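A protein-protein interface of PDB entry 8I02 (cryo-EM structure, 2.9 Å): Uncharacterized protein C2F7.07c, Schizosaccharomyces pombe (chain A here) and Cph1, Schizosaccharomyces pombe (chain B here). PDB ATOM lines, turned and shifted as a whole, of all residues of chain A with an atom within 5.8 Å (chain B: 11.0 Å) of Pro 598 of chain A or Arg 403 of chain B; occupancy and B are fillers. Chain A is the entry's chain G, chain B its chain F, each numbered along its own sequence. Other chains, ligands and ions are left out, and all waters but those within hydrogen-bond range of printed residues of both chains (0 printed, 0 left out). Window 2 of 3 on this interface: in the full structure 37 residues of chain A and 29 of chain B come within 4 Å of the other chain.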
ATOM      1  N   ASP A 569       2.761  13.681 -16.321  1.00  0.00           N
ATOM      2  CA  ASP A 569       2.144  13.083 -17.502  1.00  0.00           C
ATOM      3  C   ASP A 569       2.632  13.754 -18.783  1.00  0.00           C
ATOM      4  O   ASP A 569       1.877  14.385 -19.519  1.00  0.00           O
ATOM      5  CB  ASP A 569       0.623  13.133 -17.407  1.00  0.00           C
ATOM      6  CG  ASP A 569      -0.014  11.901 -17.949  1.00  0.00           C
ATOM      7  OD1 ASP A 569       0.726  10.955 -18.281  1.00  0.00           O
ATOM      8  OD2 ASP A 569      -1.253  11.884 -18.053  1.00  0.00           O
ATOM      9  N   LEU A 571       3.521  13.406 -22.235  1.00  0.00           N
ATOM     10  CA  LEU A 571       3.395  12.519 -23.380  1.00  0.00           C
ATOM     11  C   LEU A 571       4.497  12.738 -24.402  1.00  0.00           C
ATOM     12  O   LEU A 571       4.594  11.963 -25.357  1.00  0.00           O
ATOM     13  CB  LEU A 571       2.021  12.700 -24.019  1.00  0.00           C
ATOM     14  CG  LEU A 571       0.902  12.047 -23.219  1.00  0.00           C
ATOM     15  CD1 LEU A 571      -0.426  12.592 -23.638  1.00  0.00           C
ATOM     16  CD2 LEU A 571       0.954  10.553 -23.409  1.00  0.00           C
ATOM     17  N   TYR A 576       8.113   7.262 -22.083  1.00  0.00           N
ATOM     18  CA  TYR A 576       6.927   7.079 -21.257  1.00  0.00           C
ATOM     19  C   TYR A 576       5.850   6.324 -22.019  1.00  0.00           C
ATOM     20  O   TYR A 576       5.322   5.314 -21.538  1.00  0.00           O
ATOM     21  CB  TYR A 576       6.426   8.454 -20.819  1.00  0.00           C
ATOM     22  CG  TYR A 576       5.201   8.514 -19.946  1.00  0.00           C
ATOM     23  CD1 TYR A 576       4.410   9.642 -19.942  1.00  0.00           C
ATOM     24  CD2 TYR A 576       4.850   7.477 -19.112  1.00  0.00           C
ATOM     25  CE1 TYR A 576       3.301   9.732 -19.153  1.00  0.00           C
ATOM     26  CE2 TYR A 576       3.732   7.560 -18.316  1.00  0.00           C
ATOM     27  CZ  TYR A 576       2.965   8.692 -18.342  1.00  0.00           C
ATOM     28  OH  TYR A 576       1.851   8.784 -17.553  1.00  0.00           O
ATOM     29  N   LEU A 580       3.596   2.883 -21.574  1.00  0.00           N
ATOM     30  CA  LEU A 580       2.148   2.836 -21.741  1.00  0.00           C
ATOM     31  C   LEU A 580       1.730   1.796 -22.780  1.00  0.00           C
ATOM     32  O   LEU A 580       0.702   1.127 -22.627  1.00  0.00           O
ATOM     33  CB  LEU A 580       1.638   4.218 -22.121  1.00  0.00           C
ATOM     34  CG  LEU A 580       1.823   5.276 -21.044  1.00  0.00           C
ATOM     35  CD1 LEU A 580       1.136   6.568 -21.417  1.00  0.00           C
ATOM     36  CD2 LEU A 580       1.300   4.775 -19.734  1.00  0.00           C
ATOM     37  N   PRO A 596      -7.804   4.202 -22.709  1.00  0.00           N
ATOM     38  CA  PRO A 596      -8.149   5.112 -21.620  1.00  0.00           C
ATOM     39  C   PRO A 596      -7.088   6.190 -21.450  1.00  0.00           C
ATOM     40  O   PRO A 596      -5.967   6.081 -21.946  1.00  0.00           O
ATOM     41  CB  PRO A 596      -8.200   4.182 -20.400  1.00  0.00           C
ATOM     42  CG  PRO A 596      -7.659   2.833 -20.879  1.00  0.00           C
ATOM     43  CD  PRO A 596      -7.065   3.035 -22.214  1.00  0.00           C
ATOM     44  N   ALA A 597      -7.471   7.250 -20.744  1.00  0.00           N
ATOM     45  CA  ALA A 597      -6.548   8.335 -20.437  1.00  0.00           C
ATOM     46  C   ALA A 597      -5.305   7.744 -19.785  1.00  0.00           C
ATOM     47  O   ALA A 597      -5.398   6.702 -19.131  1.00  0.00           O
ATOM     48  CB  ALA A 597      -7.221   9.367 -19.536  1.00  0.00           C
ATOM     49  N   PRO A 598      -4.128   8.351 -19.948  1.00  0.00           N
ATOM     50  CA  PRO A 598      -2.895   7.649 -19.550  1.00  0.00           C
ATOM     51  C   PRO A 598      -2.817   7.335 -18.067  1.00  0.00           C
ATOM     52  O   PRO A 598      -2.117   6.392 -17.681  1.00  0.00           O
ATOM     53  CB  PRO A 598      -1.789   8.614 -19.998  1.00  0.00           C
ATOM     54  CG  PRO A 598      -2.445   9.916 -20.126  1.00  0.00           C
ATOM     55  CD  PRO A 598      -3.845   9.671 -20.523  1.00  0.00           C
ATOM     56  N   PHE A 599      -3.520   8.093 -17.225  1.00  0.00           N
ATOM     57  CA  PHE A 599      -3.603   7.785 -15.803  1.00  0.00           C
ATOM     58  C   PHE A 599      -4.533   6.611 -15.520  1.00  0.00           C
ATOM     59  O   PHE A 599      -4.287   5.850 -14.579  1.00  0.00           O
ATOM     60  CB  PHE A 599      -4.087   9.010 -15.027  1.00  0.00           C
ATOM     61  CG  PHE A 599      -2.994   9.978 -14.646  1.00  0.00           C
ATOM     62  CD1 PHE A 599      -3.294  11.299 -14.360  1.00  0.00           C
ATOM     63  CD2 PHE A 599      -1.677   9.569 -14.553  1.00  0.00           C
ATOM     64  CE1 PHE A 599      -2.313  12.187 -14.004  1.00  0.00           C
ATOM     65  CE2 PHE A 599      -0.694  10.462 -14.196  1.00  0.00           C
ATOM     66  CZ  PHE A 599      -1.017  11.770 -13.923  1.00  0.00           C
ATOM     67  N   ASP A 600      -5.601   6.448 -16.311  1.00  0.00           N
ATOM     68  CA  ASP A 600      -6.601   5.415 -16.055  1.00  0.00           C
ATOM     69  C   ASP A 600      -6.160   4.049 -16.544  1.00  0.00           C
ATOM     70  O   ASP A 600      -6.650   3.033 -16.045  1.00  0.00           O
ATOM     71  CB  ASP A 600      -7.922   5.787 -16.708  1.00  0.00           C
ATOM     72  CG  ASP A 600      -8.467   7.081 -16.192  1.00  0.00           C
ATOM     73  OD1 ASP A 600      -7.756   8.099 -16.278  1.00  0.00           O
ATOM     74  OD2 ASP A 600      -9.604   7.086 -15.690  1.00  0.00           O
ATOM     75  N   LEU A 601      -5.278   3.997 -17.530  1.00  0.00           N
ATOM     76  CA  LEU A 601      -4.630   2.742 -17.865  1.00  0.00           C
ATOM     77  C   LEU A 601      -3.701   2.292 -16.749  1.00  0.00           C
ATOM     78  O   LEU A 601      -3.468   1.089 -16.585  1.00  0.00           O
ATOM     79  CB  LEU A 601      -3.875   2.912 -19.178  1.00  0.00           C
ATOM     80  CG  LEU A 601      -3.021   1.790 -19.739  1.00  0.00           C
ATOM     81  CD1 LEU A 601      -3.895   0.683 -20.217  1.00  0.00           C
ATOM     82  CD2 LEU A 601      -2.193   2.344 -20.861  1.00  0.00           C
ATOM     83  N   ALA A 602      -3.194   3.233 -15.955  1.00  0.00           N
ATOM     84  CA  ALA A 602      -2.304   2.936 -14.843  1.00  0.00           C
ATOM     85  C   ALA A 602      -3.017   2.260 -13.685  1.00  0.00           C
ATOM     86  O   ALA A 602      -2.355   1.831 -12.738  1.00  0.00           O
ATOM     87  CB  ALA A 602      -1.624   4.216 -14.360  1.00  0.00           C
ATOM     88  N   ALA B 394       2.458   8.008 -33.061  1.00  0.00           N
ATOM     89  CA  ALA B 394       1.182   7.303 -33.026  1.00  0.00           C
ATOM     90  C   ALA B 394       0.663   7.199 -31.599  1.00  0.00           C
ATOM     91  O   ALA B 394      -0.482   7.573 -31.305  1.00  0.00           O
ATOM     92  CB  ALA B 394       1.344   5.914 -33.635  1.00  0.00           C
ATOM     93  N   LEU B 395       1.502   6.683 -30.695  1.00  0.00           N
ATOM     94  CA  LEU B 395       1.092   6.533 -29.305  1.00  0.00           C
ATOM     95  C   LEU B 395       0.735   7.876 -28.698  1.00  0.00           C
ATOM     96  O   LEU B 395      -0.258   7.996 -27.979  1.00  0.00           O
ATOM     97  CB  LEU B 395       2.200   5.860 -28.507  1.00  0.00           C
ATOM     98  CG  LEU B 395       2.431   4.401 -28.872  1.00  0.00           C
ATOM     99  CD1 LEU B 395       3.680   3.869 -28.228  1.00  0.00           C
ATOM    100  CD2 LEU B 395       1.250   3.573 -28.454  1.00  0.00           C
ATOM    101  N   ARG B 396       1.530   8.898 -28.985  1.00  0.00           N
ATOM    102  CA  ARG B 396       1.285  10.212 -28.412  1.00  0.00           C
ATOM    103  C   ARG B 396      -0.064  10.753 -28.841  1.00  0.00           C
ATOM    104  O   ARG B 396      -0.833  11.266 -28.020  1.00  0.00           O
ATOM    105  CB  ARG B 396       2.395  11.167 -28.823  1.00  0.00           C
ATOM    106  CG  ARG B 396       2.294  12.556 -28.244  1.00  0.00           C
ATOM    107  CD  ARG B 396       3.583  13.286 -28.530  1.00  0.00           C
ATOM    108  NE  ARG B 396       4.724  12.423 -28.243  1.00  0.00           N
ATOM    109  CZ  ARG B 396       5.925  12.569 -28.787  1.00  0.00           C
ATOM    110  NH1 ARG B 396       6.139  13.542 -29.656  1.00  0.00           N
ATOM    111  NH2 ARG B 396       6.909  11.738 -28.470  1.00  0.00           N
ATOM    112  N   THR B 397      -0.384  10.642 -30.126  1.00  0.00           N
ATOM    113  CA  THR B 397      -1.628  11.237 -30.585  1.00  0.00           C
ATOM    114  C   THR B 397      -2.842  10.435 -30.134  1.00  0.00           C
ATOM    115  O   THR B 397      -3.875  11.029 -29.829  1.00  0.00           O
ATOM    116  CB  THR B 397      -1.606  11.411 -32.097  1.00  0.00           C
ATOM    117  OG1 THR B 397      -2.760  12.149 -32.507  1.00  0.00           O
ATOM    118  CG2 THR B 397      -1.570  10.078 -32.786  1.00  0.00           C
ATOM    119  N   LEU B 398      -2.741   9.108 -30.015  1.00  0.00           N
ATOM    120  CA  LEU B 398      -3.920   8.388 -29.534  1.00  0.00           C
ATOM    121  C   LEU B 398      -4.103   8.516 -28.025  1.00  0.00           C
ATOM    122  O   LEU B 398      -5.248   8.540 -27.549  1.00  0.00           O
ATOM    123  CB  LEU B 398      -3.880   6.921 -29.965  1.00  0.00           C
ATOM    124  CG  LEU B 398      -2.900   5.909 -29.414  1.00  0.00           C
ATOM    125  CD1 LEU B 398      -3.562   5.095 -28.354  1.00  0.00           C
ATOM    126  CD2 LEU B 398      -2.441   5.007 -30.518  1.00  0.00           C
ATOM    127  N   PHE B 399      -3.016   8.645 -27.255  1.00  0.00           N
ATOM    128  CA  PHE B 399      -3.164   8.877 -25.819  1.00  0.00           C
ATOM    129  C   PHE B 399      -3.612  10.297 -25.518  1.00  0.00           C
ATOM    130  O   PHE B 399      -4.254  10.531 -24.494  1.00  0.00           O
ATOM    131  CB  PHE B 399      -1.862   8.575 -25.097  1.00  0.00           C
ATOM    132  CG  PHE B 399      -1.698   7.140 -24.736  1.00  0.00           C
ATOM    133  CD1 PHE B 399      -2.614   6.513 -23.928  1.00  0.00           C
ATOM    134  CD2 PHE B 399      -0.622   6.421 -25.193  1.00  0.00           C
ATOM    135  CE1 PHE B 399      -2.460   5.197 -23.596  1.00  0.00           C
ATOM    136  CE2 PHE B 399      -0.470   5.106 -24.863  1.00  0.00           C
ATOM    137  CZ  PHE B 399      -1.387   4.498 -24.064  1.00  0.00           C
ATOM    138  N   ASN B 400      -3.287  11.259 -26.380  1.00  0.00           N
ATOM    139  CA  ASN B 400      -3.853  12.594 -26.237  1.00  0.00           C
ATOM    140  C   ASN B 400      -5.277  12.659 -26.770  1.00  0.00           C
ATOM    141  O   ASN B 400      -6.049  13.532 -26.365  1.00  0.00           O
ATOM    142  CB  ASN B 400      -2.971  13.613 -26.951  1.00  0.00           C
ATOM    143  CG  ASN B 400      -3.196  15.026 -26.463  1.00  0.00           C
ATOM    144  OD1 ASN B 400      -4.328  15.485 -26.351  1.00  0.00           O
ATOM    145  ND2 ASN B 400      -2.110  15.729 -26.174  1.00  0.00           N
ATOM    146  N   LYS B 401      -5.634  11.765 -27.692  1.00  0.00           N
ATOM    147  CA  LYS B 401      -7.033  11.576 -28.058  1.00  0.00           C
ATOM    148  C   LYS B 401      -7.854  11.161 -26.846  1.00  0.00           C
ATOM    149  O   LYS B 401      -8.793  11.857 -26.441  1.00  0.00           O
ATOM    150  CB  LYS B 401      -7.140  10.513 -29.148  1.00  0.00           C
ATOM    151  CG  LYS B 401      -6.845  10.987 -30.550  1.00  0.00           C
ATOM    152  CD  LYS B 401      -7.733  10.278 -31.558  1.00  0.00           C
ATOM    153  CE  LYS B 401      -9.181  10.715 -31.446  1.00  0.00           C
ATOM    154  NZ  LYS B 401     -10.007  10.161 -32.554  1.00  0.00           N
ATOM    155  N   ALA B 402      -7.492  10.025 -26.243  1.00  0.00           N
ATOM    156  CA  ALA B 402      -8.292   9.463 -25.162  1.00  0.00           C
ATOM    157  C   ALA B 402      -8.335  10.369 -23.942  1.00  0.00           C
ATOM    158  O   ALA B 402      -9.304  10.337 -23.180  1.00  0.00           O
ATOM    159  CB  ALA B 402      -7.743   8.096 -24.777  1.00  0.00           C
ATOM    160  N   ARG B 403      -7.308  11.177 -23.736  1.00  0.00           N
ATOM    161  CA  ARG B 403      -7.215  12.040 -22.562  1.00  0.00           C
ATOM    162  C   ARG B 403      -7.955  13.336 -22.859  1.00  0.00           C
ATOM    163  O   ARG B 403      -7.433  14.216 -23.546  1.00  0.00           O
ATOM    164  CB  ARG B 403      -5.756  12.300 -22.213  1.00  0.00           C
ATOM    165  CG  ARG B 403      -5.531  12.823 -20.825  1.00  0.00           C
ATOM    166  CD  ARG B 403      -4.097  13.233 -20.664  1.00  0.00           C
ATOM    167  NE  ARG B 403      -3.797  14.406 -21.471  1.00  0.00           N
ATOM    168  CZ  ARG B 403      -2.574  14.872 -21.671  1.00  0.00           C
ATOM    169  NH1 ARG B 403      -1.538  14.260 -21.121  1.00  0.00           N
ATOM    170  NH2 ARG B 403      -2.386  15.948 -22.422  1.00  0.00           N
ATOM    171  N   THR B 404      -9.169  13.455 -22.336  1.00  0.00           N
ATOM    172  CA  THR B 404     -10.011  14.636 -22.547  1.00  0.00           C
ATOM    173  C   THR B 404     -10.265  14.898 -24.029  1.00  0.00           C
ATOM    174  O   THR B 404     -10.500  16.036 -24.437  1.00  0.00           O
ATOM    175  CB  THR B 404      -9.391  15.896 -21.921  1.00  0.00           C
ATOM    176  OG1 THR B 404      -8.217  16.268 -22.654  1.00  0.00           O
ATOM    177  CG2 THR B 404      -9.015  15.636 -20.475  1.00  0.00           C
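Of the 11 printed residues of chain A, 6 touch a printed residue of chain B. Printed residues of chain A that touch a printed residue of chain B: Asp 569, Leu 571, Leu 580, Pro 596, Pro 598 and Leu 601. Along chain A the printed residues that touch a printed residue of chain B span positions 569 to 601. Of the 11 printed residues of chain B, 4 touch a printed residue of chain A. Printed residues of chain B that touch a printed residue of chain A: Arg 396, Phe 399, Ala 402 and Arg 403. Hydrophobic or aromatic side chains of chain B that line the printed part of chain A: Phe 399 and Ala 402. Among the printed residues, 9 pairs touch across the chains. Among the printed residues, Asp or Glu carboxylates within 4 Å of a Lys or Arg side-chain nitrogen of the other chain: Asp 569 of chain A with Arg 403 of chain B (3.9 Å).
The side-chain carboxylate (OD1) of Asp 569 of chain A sits at hydrogen-bond distance from the side-chain hydroxyl (OH) of Tyr 576 of chain A (2.6 Å).
Leu 571 of chain A touches Phe 399 of chain B (CD2 to CB, 3.8 Å). Leu 571 of chain A touches Arg 403 of chain B. CB of Leu 580 of chain A touches CE2 of Phe 399 of chain B, 3.6 Å away. Phe 399 of chain B touches Pro 596 of chain A. Ala 402 of chain B touches Pro 596 of chain A. Arg 403 of chain B touches Pro 598 of chain A. Phe 399 of chain B touches Leu 601 of chain A (CZ to CD2, 3.9 Å).
The guanidinium group (NE) of Arg 396 of chain B lies within hydrogen-bond range of the backbone carbonyl oxygen (O) of Leu 571 of chain A, at 2.9 Å. NH1 of Arg 403 of chain B is in salt-bridge range of OD2 of Asp 569 of chain A (3.9 Å).
Asp 569 of chain A touches one residue of chain B. Printed residues of chain B within 4 Å of Leu 571 of chain A: Arg 396 (2.9 Å), Phe 399 (3.8 Å) and Arg 403 (3.2 Å). Printed residues of chain B within 4 Å of Leu 580 of chain A: Phe 399. No residue of chain B comes within 4 Å of Ala 597 of chain A. Pro 598 of chain A touches one residue of chain B. No residue of chain B comes within 4 Å of Phe 599 of chain A. Of chain B, only Phe 399 (3.9 Å) comes within 4 Å of Leu 601 of chain A. Of the printed residues of chain A, Arg 396 of chain B touches Leu 571 (2.9 Å). Of the printed residues of chain A, Phe 399 of chain B touches Leu 571, Leu 580, Pro 596 and Leu 601. Of the printed residues of chain A, Ala 402 of chain B touches Pro 596. Arg 403 of chain B touches three residues of chain A. The nearest residue of chain B that does not touch Pro 598 of chain A is Phe 399 of chain B (4.1 Å). The nearest residue of chain A that does not touch Arg 403 of chain B is Ala 597 of chain A (4.04 Å). The nearest printed residue of chain B that does not touch Leu 580 of chain A is Leu 395 of chain B (6.0 Å).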
